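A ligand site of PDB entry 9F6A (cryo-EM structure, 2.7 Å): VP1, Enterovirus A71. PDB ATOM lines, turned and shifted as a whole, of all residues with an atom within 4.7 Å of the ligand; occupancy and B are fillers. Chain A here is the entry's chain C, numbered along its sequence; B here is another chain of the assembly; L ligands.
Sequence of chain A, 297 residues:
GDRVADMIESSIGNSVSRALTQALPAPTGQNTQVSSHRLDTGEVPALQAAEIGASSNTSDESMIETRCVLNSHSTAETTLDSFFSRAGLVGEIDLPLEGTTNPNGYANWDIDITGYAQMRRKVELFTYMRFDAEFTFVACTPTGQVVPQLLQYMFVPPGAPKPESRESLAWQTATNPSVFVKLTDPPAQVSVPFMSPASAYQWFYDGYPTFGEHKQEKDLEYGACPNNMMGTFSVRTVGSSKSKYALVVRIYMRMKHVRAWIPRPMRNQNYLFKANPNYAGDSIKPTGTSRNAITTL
O2 of the ligand is in hydrogen-bond range of N of Ile 113, at 2.8 Å.
N1 of the ligand lies within salt-bridge range of OD2 of Asp 112.
An oxygen (O2) of the ligand sits at hydrogen-bond distance from the backbone NH (N) of Thr 114 (3.3 Å).
Ile 111 touches the ligand.
Phe 135 touches the ligand (CE1 to C11, 3.5 Å).
Phe 137 touches the ligand.
Phe 155 touches the ligand.
CG2 of Val 192 touches C16 of the ligand, at 3.7 Å.
Met 195 touches the ligand (CE to C12, 3.7 Å).
Tyr 201 touches the ligand.
Trp 203 touches the ligand.
Asn 228 touches the ligand (O to C5, 3.3 Å).
CD1 of Phe 233 touches C17 of the ligand, 3.7 Å away.
Ala 275 touches the ligand (CB to O1, 3.4 Å).
Ile 24 of chain B touches the ligand.
Hydrophobic or aromatic side chains within 4 Å of the ligand: Ile 111, Ile 113, Phe 135, Phe 137, Phe 155, Val 192, Met 195, Tyr 201, Trp 203, Phe 233, Ala 275 and Ile 24 of chain B.
Within 4 Å of the ligand: Ile 111, Asp 112, Ile 113, Thr 114, Phe 135, Phe 137, Phe 155, Val 192, Met 195, Tyr 201, Trp 203, Asn 228, Phe 233, Ala 275 and Ile 24 of chain B.
The nearest printed residue that does not touch the ligand is Val 190 (4.04 Å).
N of Met 195 is in hydrogen-bond range of OH of Tyr 201 (3.1 Å).
The side-chain amide nitrogen of Asn 228 sits at hydrogen-bond distance from the backbone carbonyl oxygen of Gln 202 (2.5 Å).
OG1 of Thr 114 sits at hydrogen-bond distance from N of Ala 275, at 2.8 Å.
N of Phe 135 is in hydrogen-bond range of O of Val 190 (2.8 Å).
The side-chain carboxylate of Asp 112 lies close to the backbone NH of Thr 114 (3.4 Å).
OH of Tyr 201 sits at hydrogen-bond distance from SD of Met 230 (3.6 Å).
The backbone NH of Phe 155 is in hydrogen-bond range of the backbone carbonyl oxygen of Pro 177, at 2.7 Å.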
ATOM      1  N   ILE A 111       3.333 -23.798 -13.220  1.00  0.00           N
ATOM      2  CA  ILE A 111       3.969 -24.643 -12.222  1.00  0.00           C
ATOM      3  C   ILE A 111       2.963 -24.883 -11.101  1.00  0.00           C
ATOM      4  O   ILE A 111       2.669 -23.983 -10.297  1.00  0.00           O
ATOM      5  CB  ILE A 111       5.261 -24.023 -11.686  1.00  0.00           C
ATOM      6  CG1 ILE A 111       6.317 -23.999 -12.792  1.00  0.00           C
ATOM      7  CG2 ILE A 111       5.794 -24.823 -10.507  1.00  0.00           C
ATOM      8  CD1 ILE A 111       7.269 -22.837 -12.698  1.00  0.00           C
ATOM      9  N   ASP A 112       2.413 -26.096 -11.064  1.00  0.00           N
ATOM     10  CA  ASP A 112       1.405 -26.459 -10.064  1.00  0.00           C
ATOM     11  C   ASP A 112       1.536 -27.973  -9.857  1.00  0.00           C
ATOM     12  O   ASP A 112       1.035 -28.757 -10.670  1.00  0.00           O
ATOM     13  CB  ASP A 112       0.011 -26.068 -10.527  1.00  0.00           C
ATOM     14  CG  ASP A 112      -1.010 -26.127  -9.417  1.00  0.00           C
ATOM     15  OD1 ASP A 112      -1.560 -27.223  -9.166  1.00  0.00           O
ATOM     16  OD2 ASP A 112      -1.266 -25.086  -8.782  1.00  0.00           O
ATOM     17  N   ILE A 113       2.207 -28.357  -8.768  1.00  0.00           N
ATOM     18  CA  ILE A 113       2.499 -29.769  -8.527  1.00  0.00           C
ATOM     19  C   ILE A 113       1.310 -30.528  -7.956  1.00  0.00           C
ATOM     20  O   ILE A 113       1.447 -31.726  -7.643  1.00  0.00           O
ATOM     21  CB  ILE A 113       3.714 -29.912  -7.579  1.00  0.00           C
ATOM     22  CG1 ILE A 113       3.344 -29.455  -6.166  1.00  0.00           C
ATOM     23  CG2 ILE A 113       4.878 -29.100  -8.117  1.00  0.00           C
ATOM     24  CD1 ILE A 113       4.499 -29.521  -5.198  1.00  0.00           C
ATOM     25  N   THR A 114       0.161 -29.885  -7.805  1.00  0.00           N
ATOM     26  CA  THR A 114      -1.049 -30.537  -7.314  1.00  0.00           C
ATOM     27  C   THR A 114      -1.865 -31.183  -8.429  1.00  0.00           C
ATOM     28  O   THR A 114      -3.073 -31.367  -8.273  1.00  0.00           O
ATOM     29  CB  THR A 114      -1.918 -29.525  -6.551  1.00  0.00           C
ATOM     30  OG1 THR A 114      -2.253 -28.436  -7.404  1.00  0.00           O
ATOM     31  CG2 THR A 114      -1.178 -29.006  -5.328  1.00  0.00           C
ATOM     32  N   PHE A 131      11.494 -26.059   0.644  1.00  0.00           N
ATOM     33  CA  PHE A 131      12.417 -27.036   0.106  1.00  0.00           C
ATOM     34  C   PHE A 131      13.075 -26.481  -1.153  1.00  0.00           C
ATOM     35  O   PHE A 131      12.585 -25.529  -1.762  1.00  0.00           O
ATOM     36  CB  PHE A 131      11.701 -28.356  -0.226  1.00  0.00           C
ATOM     37  CG  PHE A 131      10.471 -28.187  -1.066  1.00  0.00           C
ATOM     38  CD1 PHE A 131      10.558 -28.107  -2.446  1.00  0.00           C
ATOM     39  CD2 PHE A 131       9.219 -28.113  -0.485  1.00  0.00           C
ATOM     40  CE1 PHE A 131       9.434 -27.943  -3.219  1.00  0.00           C
ATOM     41  CE2 PHE A 131       8.087 -27.959  -1.256  1.00  0.00           C
ATOM     42  CZ  PHE A 131       8.204 -27.874  -2.629  1.00  0.00           C
ATOM     43  N   PHE A 135      14.339 -30.910 -10.346  1.00  0.00           N
ATOM     44  CA  PHE A 135      13.340 -31.070 -11.395  1.00  0.00           C
ATOM     45  C   PHE A 135      13.944 -31.839 -12.552  1.00  0.00           C
ATOM     46  O   PHE A 135      14.996 -31.462 -13.079  1.00  0.00           O
ATOM     47  CB  PHE A 135      12.845 -29.705 -11.861  1.00  0.00           C
ATOM     48  CG  PHE A 135      11.560 -29.277 -11.219  1.00  0.00           C
ATOM     49  CD1 PHE A 135      11.552 -28.614 -10.002  1.00  0.00           C
ATOM     50  CD2 PHE A 135      10.343 -29.530 -11.833  1.00  0.00           C
ATOM     51  CE1 PHE A 135      10.368 -28.222  -9.420  1.00  0.00           C
ATOM     52  CE2 PHE A 135       9.160 -29.138 -11.250  1.00  0.00           C
ATOM     53  CZ  PHE A 135       9.172 -28.484 -10.043  1.00  0.00           C
ATOM     54  N   PHE A 137      13.027 -33.686 -16.360  1.00  0.00           N
ATOM     55  CA  PHE A 137      12.087 -33.654 -17.475  1.00  0.00           C
ATOM     56  C   PHE A 137      12.423 -34.787 -18.423  1.00  0.00           C
ATOM     57  O   PHE A 137      13.457 -34.738 -19.116  1.00  0.00           O
ATOM     58  CB  PHE A 137      12.123 -32.299 -18.171  1.00  0.00           C
ATOM     59  CG  PHE A 137      12.358 -31.137 -17.248  1.00  0.00           C
ATOM     60  CD1 PHE A 137      11.334 -30.672 -16.432  1.00  0.00           C
ATOM     61  CD2 PHE A 137      13.597 -30.530 -17.174  1.00  0.00           C
ATOM     62  CE1 PHE A 137      11.549 -29.615 -15.570  1.00  0.00           C
ATOM     63  CE2 PHE A 137      13.811 -29.475 -16.322  1.00  0.00           C
ATOM     64  CZ  PHE A 137      12.787 -29.011 -15.517  1.00  0.00           C
ATOM     65  N   PHE A 155      12.267 -21.879 -17.812  1.00  0.00           N
ATOM     66  CA  PHE A 155      11.565 -21.415 -16.616  1.00  0.00           C
ATOM     67  C   PHE A 155      11.189 -19.958 -16.820  1.00  0.00           C
ATOM     68  O   PHE A 155      12.048 -19.109 -17.043  1.00  0.00           O
ATOM     69  CB  PHE A 155      12.442 -21.590 -15.381  1.00  0.00           C
ATOM     70  CG  PHE A 155      11.876 -20.976 -14.137  1.00  0.00           C
ATOM     71  CD1 PHE A 155      10.532 -21.113 -13.820  1.00  0.00           C
ATOM     72  CD2 PHE A 155      12.682 -20.251 -13.279  1.00  0.00           C
ATOM     73  CE1 PHE A 155      10.013 -20.540 -12.683  1.00  0.00           C
ATOM     74  CE2 PHE A 155      12.173 -19.677 -12.143  1.00  0.00           C
ATOM     75  CZ  PHE A 155      10.829 -19.817 -11.845  1.00  0.00           C
ATOM     76  N   PRO A 177      15.994 -18.677 -16.816  1.00  0.00           N
ATOM     77  CA  PRO A 177      16.725 -19.951 -16.815  1.00  0.00           C
ATOM     78  C   PRO A 177      16.091 -20.909 -17.814  1.00  0.00           C
ATOM     79  O   PRO A 177      14.896 -21.215 -17.719  1.00  0.00           O
ATOM     80  CB  PRO A 177      16.579 -20.449 -15.368  1.00  0.00           C
ATOM     81  CG  PRO A 177      16.024 -19.296 -14.595  1.00  0.00           C
ATOM     82  CD  PRO A 177      15.261 -18.463 -15.555  1.00  0.00           C
ATOM     83  N   VAL A 179      16.794 -24.553 -20.447  1.00  0.00           N
ATOM     84  CA  VAL A 179      17.559 -25.771 -20.691  1.00  0.00           C
ATOM     85  C   VAL A 179      17.399 -26.151 -22.151  1.00  0.00           C
ATOM     86  O   VAL A 179      16.279 -26.240 -22.667  1.00  0.00           O
ATOM     87  CB  VAL A 179      17.098 -26.928 -19.784  1.00  0.00           C
ATOM     88  CG1 VAL A 179      18.048 -28.096 -19.894  1.00  0.00           C
ATOM     89  CG2 VAL A 179      16.981 -26.460 -18.345  1.00  0.00           C
ATOM     90  N   VAL A 190      17.609 -30.298 -13.226  1.00  0.00           N
ATOM     91  CA  VAL A 190      18.002 -28.982 -12.754  1.00  0.00           C
ATOM     92  C   VAL A 190      17.642 -28.862 -11.282  1.00  0.00           C
ATOM     93  O   VAL A 190      16.651 -29.424 -10.817  1.00  0.00           O
ATOM     94  CB  VAL A 190      17.331 -27.855 -13.566  1.00  0.00           C
ATOM     95  CG1 VAL A 190      17.978 -27.720 -14.935  1.00  0.00           C
ATOM     96  CG2 VAL A 190      15.834 -28.077 -13.683  1.00  0.00           C
ATOM     97  N   VAL A 192      16.248 -26.600  -8.514  1.00  0.00           N
ATOM     98  CA  VAL A 192      15.391 -25.431  -8.359  1.00  0.00           C
ATOM     99  C   VAL A 192      15.408 -25.029  -6.885  1.00  0.00           C
ATOM    100  O   VAL A 192      15.133 -25.869  -6.022  1.00  0.00           O
ATOM    101  CB  VAL A 192      13.958 -25.724  -8.833  1.00  0.00           C
ATOM    102  CG1 VAL A 192      13.064 -24.526  -8.589  1.00  0.00           C
ATOM    103  CG2 VAL A 192      13.984 -26.069 -10.309  1.00  0.00           C
ATOM    104  N   MET A 195      12.040 -20.622  -3.992  1.00  0.00           N
ATOM    105  CA  MET A 195      11.866 -19.346  -4.663  1.00  0.00           C
ATOM    106  C   MET A 195      10.683 -18.544  -4.142  1.00  0.00           C
ATOM    107  O   MET A 195      10.434 -17.446  -4.646  1.00  0.00           O
ATOM    108  CB  MET A 195      11.722 -19.578  -6.170  1.00  0.00           C
ATOM    109  CG  MET A 195      12.869 -20.377  -6.762  1.00  0.00           C
ATOM    110  SD  MET A 195      12.673 -20.728  -8.509  1.00  0.00           S
ATOM    111  CE  MET A 195      10.916 -21.011  -8.572  1.00  0.00           C
ATOM    112  N   TYR A 201       6.449 -22.826   1.064  1.00  0.00           N
ATOM    113  CA  TYR A 201       5.326 -23.032   0.162  1.00  0.00           C
ATOM    114  C   TYR A 201       4.095 -23.429   0.967  1.00  0.00           C
ATOM    115  O   TYR A 201       4.199 -23.946   2.078  1.00  0.00           O
ATOM    116  CB  TYR A 201       5.646 -24.100  -0.877  1.00  0.00           C
ATOM    117  CG  TYR A 201       6.746 -23.717  -1.835  1.00  0.00           C
ATOM    118  CD1 TYR A 201       6.623 -22.612  -2.662  1.00  0.00           C
ATOM    119  CD2 TYR A 201       7.915 -24.466  -1.907  1.00  0.00           C
ATOM    120  CE1 TYR A 201       7.622 -22.261  -3.537  1.00  0.00           C
ATOM    121  CE2 TYR A 201       8.924 -24.114  -2.784  1.00  0.00           C
ATOM    122  CZ  TYR A 201       8.773 -23.012  -3.598  1.00  0.00           C
ATOM    123  OH  TYR A 201       9.783 -22.669  -4.473  1.00  0.00           O
ATOM    124  N   GLN A 202       2.927 -23.198   0.388  1.00  0.00           N
ATOM    125  CA  GLN A 202       1.682 -23.228   1.139  1.00  0.00           C
ATOM    126  C   GLN A 202       0.615 -23.900   0.275  1.00  0.00           C
ATOM    127  O   GLN A 202      -0.022 -23.252  -0.557  1.00  0.00           O
ATOM    128  CB  GLN A 202       1.283 -21.799   1.520  1.00  0.00           C
ATOM    129  CG  GLN A 202      -0.019 -21.649   2.232  1.00  0.00           C
ATOM    130  CD  GLN A 202      -0.097 -20.355   2.997  1.00  0.00           C
ATOM    131  OE1 GLN A 202      -0.682 -20.294   4.073  1.00  0.00           O
ATOM    132  NE2 GLN A 202       0.508 -19.310   2.457  1.00  0.00           N
ATOM    133  N   TRP A 203       0.445 -25.214   0.472  1.00  0.00           N
ATOM    134  CA  TRP A 203      -0.525 -25.963  -0.323  1.00  0.00           C
ATOM    135  C   TRP A 203      -1.961 -25.668   0.087  1.00  0.00           C
ATOM    136  O   TRP A 203      -2.884 -26.004  -0.670  1.00  0.00           O
ATOM    137  CB  TRP A 203      -0.271 -27.463  -0.206  1.00  0.00           C
ATOM    138  CG  TRP A 203       1.168 -27.808   0.003  1.00  0.00           C
ATOM    139  CD1 TRP A 203       1.707 -28.406   1.095  1.00  0.00           C
ATOM    140  CD2 TRP A 203       2.244 -27.595  -0.914  1.00  0.00           C
ATOM    141  NE1 TRP A 203       3.053 -28.571   0.932  1.00  0.00           N
ATOM    142  CE2 TRP A 203       3.410 -28.087  -0.299  1.00  0.00           C
ATOM    143  CE3 TRP A 203       2.334 -27.036  -2.185  1.00  0.00           C
ATOM    144  CZ2 TRP A 203       4.652 -28.035  -0.911  1.00  0.00           C
ATOM    145  CZ3 TRP A 203       3.576 -26.983  -2.797  1.00  0.00           C
ATOM    146  CH2 TRP A 203       4.714 -27.476  -2.161  1.00  0.00           C
ATOM    147  N   ASN A 228       2.830 -19.366  -4.139  1.00  0.00           N
ATOM    148  CA  ASN A 228       3.011 -20.702  -4.687  1.00  0.00           C
ATOM    149  C   ASN A 228       3.063 -20.742  -6.208  1.00  0.00           C
ATOM    150  O   ASN A 228       3.818 -21.541  -6.758  1.00  0.00           O
ATOM    151  CB  ASN A 228       1.899 -21.638  -4.212  1.00  0.00           C
ATOM    152  CG  ASN A 228       2.207 -22.260  -2.869  1.00  0.00           C
ATOM    153  OD1 ASN A 228       3.103 -21.824  -2.159  1.00  0.00           O
ATOM    154  ND2 ASN A 228       1.486 -23.318  -2.546  1.00  0.00           N
ATOM    155  N   MET A 229       2.253 -19.944  -6.905  1.00  0.00           N
ATOM    156  CA  MET A 229       2.389 -19.889  -8.354  1.00  0.00           C
ATOM    157  C   MET A 229       3.670 -19.163  -8.710  1.00  0.00           C
ATOM    158  O   MET A 229       3.847 -17.986  -8.386  1.00  0.00           O
ATOM    159  CB  MET A 229       1.183 -19.205  -9.011  1.00  0.00           C
ATOM    160  CG  MET A 229       0.634 -17.981  -8.311  1.00  0.00           C
ATOM    161  SD  MET A 229      -1.164 -18.056  -8.134  1.00  0.00           S
ATOM    162  CE  MET A 229      -1.368 -19.426  -7.010  1.00  0.00           C
ATOM    163  N   MET A 230       4.577 -19.875  -9.365  1.00  0.00           N
ATOM    164  CA  MET A 230       5.914 -19.377  -9.664  1.00  0.00           C
ATOM    165  C   MET A 230       6.122 -19.289 -11.164  1.00  0.00           C
ATOM    166  O   MET A 230       7.149 -19.697 -11.705  1.00  0.00           O
ATOM    167  CB  MET A 230       6.973 -20.247  -9.008  1.00  0.00           C
ATOM    168  CG  MET A 230       6.709 -20.461  -7.534  1.00  0.00           C
ATOM    169  SD  MET A 230       8.123 -20.158  -6.492  1.00  0.00           S
ATOM    170  CE  MET A 230       7.837 -18.420  -6.201  1.00  0.00           C
ATOM    171  N   PHE A 233       6.327 -23.110 -16.810  1.00  0.00           N
ATOM    172  CA  PHE A 233       7.445 -23.881 -17.333  1.00  0.00           C
ATOM    173  C   PHE A 233       7.186 -24.075 -18.821  1.00  0.00           C
ATOM    174  O   PHE A 233       6.321 -24.854 -19.219  1.00  0.00           O
ATOM    175  CB  PHE A 233       7.571 -25.217 -16.609  1.00  0.00           C
ATOM    176  CG  PHE A 233       8.553 -26.157 -17.227  1.00  0.00           C
ATOM    177  CD1 PHE A 233       9.910 -25.901 -17.150  1.00  0.00           C
ATOM    178  CD2 PHE A 233       8.123 -27.303 -17.879  1.00  0.00           C
ATOM    179  CE1 PHE A 233      10.825 -26.761 -17.718  1.00  0.00           C
ATOM    180  CE2 PHE A 233       9.028 -28.165 -18.447  1.00  0.00           C
ATOM    181  CZ  PHE A 233      10.384 -27.899 -18.371  1.00  0.00           C
ATOM    182  N   ALA A 275      -4.811 -27.415  -6.860  1.00  0.00           N
ATOM    183  CA  ALA A 275      -4.804 -26.329  -5.881  1.00  0.00           C
ATOM    184  C   ALA A 275      -6.217 -26.061  -5.346  1.00  0.00           C
ATOM    185  O   ALA A 275      -6.632 -24.913  -5.158  1.00  0.00           O
ATOM    186  CB  ALA A 275      -4.182 -25.052  -6.461  1.00  0.00           C
ATOM    187  N   ILE B  24      19.426 -23.661 -11.490  1.00  0.00           N
ATOM    188  CA  ILE B  24      18.855 -22.790 -12.517  1.00  0.00           C
ATOM    189  C   ILE B  24      19.163 -21.337 -12.248  1.00  0.00           C
ATOM    190  O   ILE B  24      19.381 -20.557 -13.178  1.00  0.00           O
ATOM    191  CB  ILE B  24      17.338 -23.017 -12.642  1.00  0.00           C
ATOM    192  CG1 ILE B  24      16.685 -23.099 -11.262  1.00  0.00           C
ATOM    193  CG2 ILE B  24      17.037 -24.235 -13.471  1.00  0.00           C
ATOM    194  CD1 ILE B  24      15.253 -22.601 -11.234  1.00  0.00           C
HETATM  195  C1  LIG L   1      -0.817 -25.069  -4.163  1.00  0.00           C
HETATM  196  O1  LIG L   1      -1.927 -25.924  -4.058  1.00  0.00           O
HETATM  197  C2  LIG L   1      -0.264 -25.089  -5.581  1.00  0.00           C
HETATM  198  N1  LIG L   1       0.046 -23.741  -6.005  1.00  0.00           N
HETATM  199  C3  LIG L   1       0.958 -26.009  -5.677  1.00  0.00           C
HETATM  200  O2  LIG L   1       0.914 -26.785  -6.851  1.00  0.00           O
HETATM  201  C4  LIG L   1       2.292 -25.326  -5.540  1.00  0.00           C
HETATM  202  C5  LIG L   1       2.960 -24.713  -6.699  1.00  0.00           C
HETATM  203  C6  LIG L   1       4.452 -24.838  -6.877  1.00  0.00           C
HETATM  204  C7  LIG L   1       5.097 -25.282  -5.572  1.00  0.00           C
HETATM  205  C8  LIG L   1       6.595 -24.972  -5.542  1.00  0.00           C
HETATM  206  C9  LIG L   1       7.367 -25.564  -6.708  1.00  0.00           C
HETATM  207  C10 LIG L   1       8.111 -24.474  -7.476  1.00  0.00           C
HETATM  208  C11 LIG L   1       9.144 -25.072  -8.422  1.00  0.00           C
HETATM  209  C12 LIG L   1       9.396 -24.180  -9.627  1.00  0.00           C
HETATM  210  C13 LIG L   1       9.737 -24.991 -10.865  1.00  0.00           C
HETATM  211  C14 LIG L   1      10.913 -24.402 -11.639  1.00  0.00           C
HETATM  212  C15 LIG L   1      11.315 -25.313 -12.792  1.00  0.00           C
HETATM  213  C16 LIG L   1      12.584 -24.841 -13.489  1.00  0.00           C
HETATM  214  C17 LIG L   1      12.732 -25.497 -14.856  1.00  0.00           C
HETATM  215  C18 LIG L   1      13.988 -25.020 -15.574  1.00  0.00           C
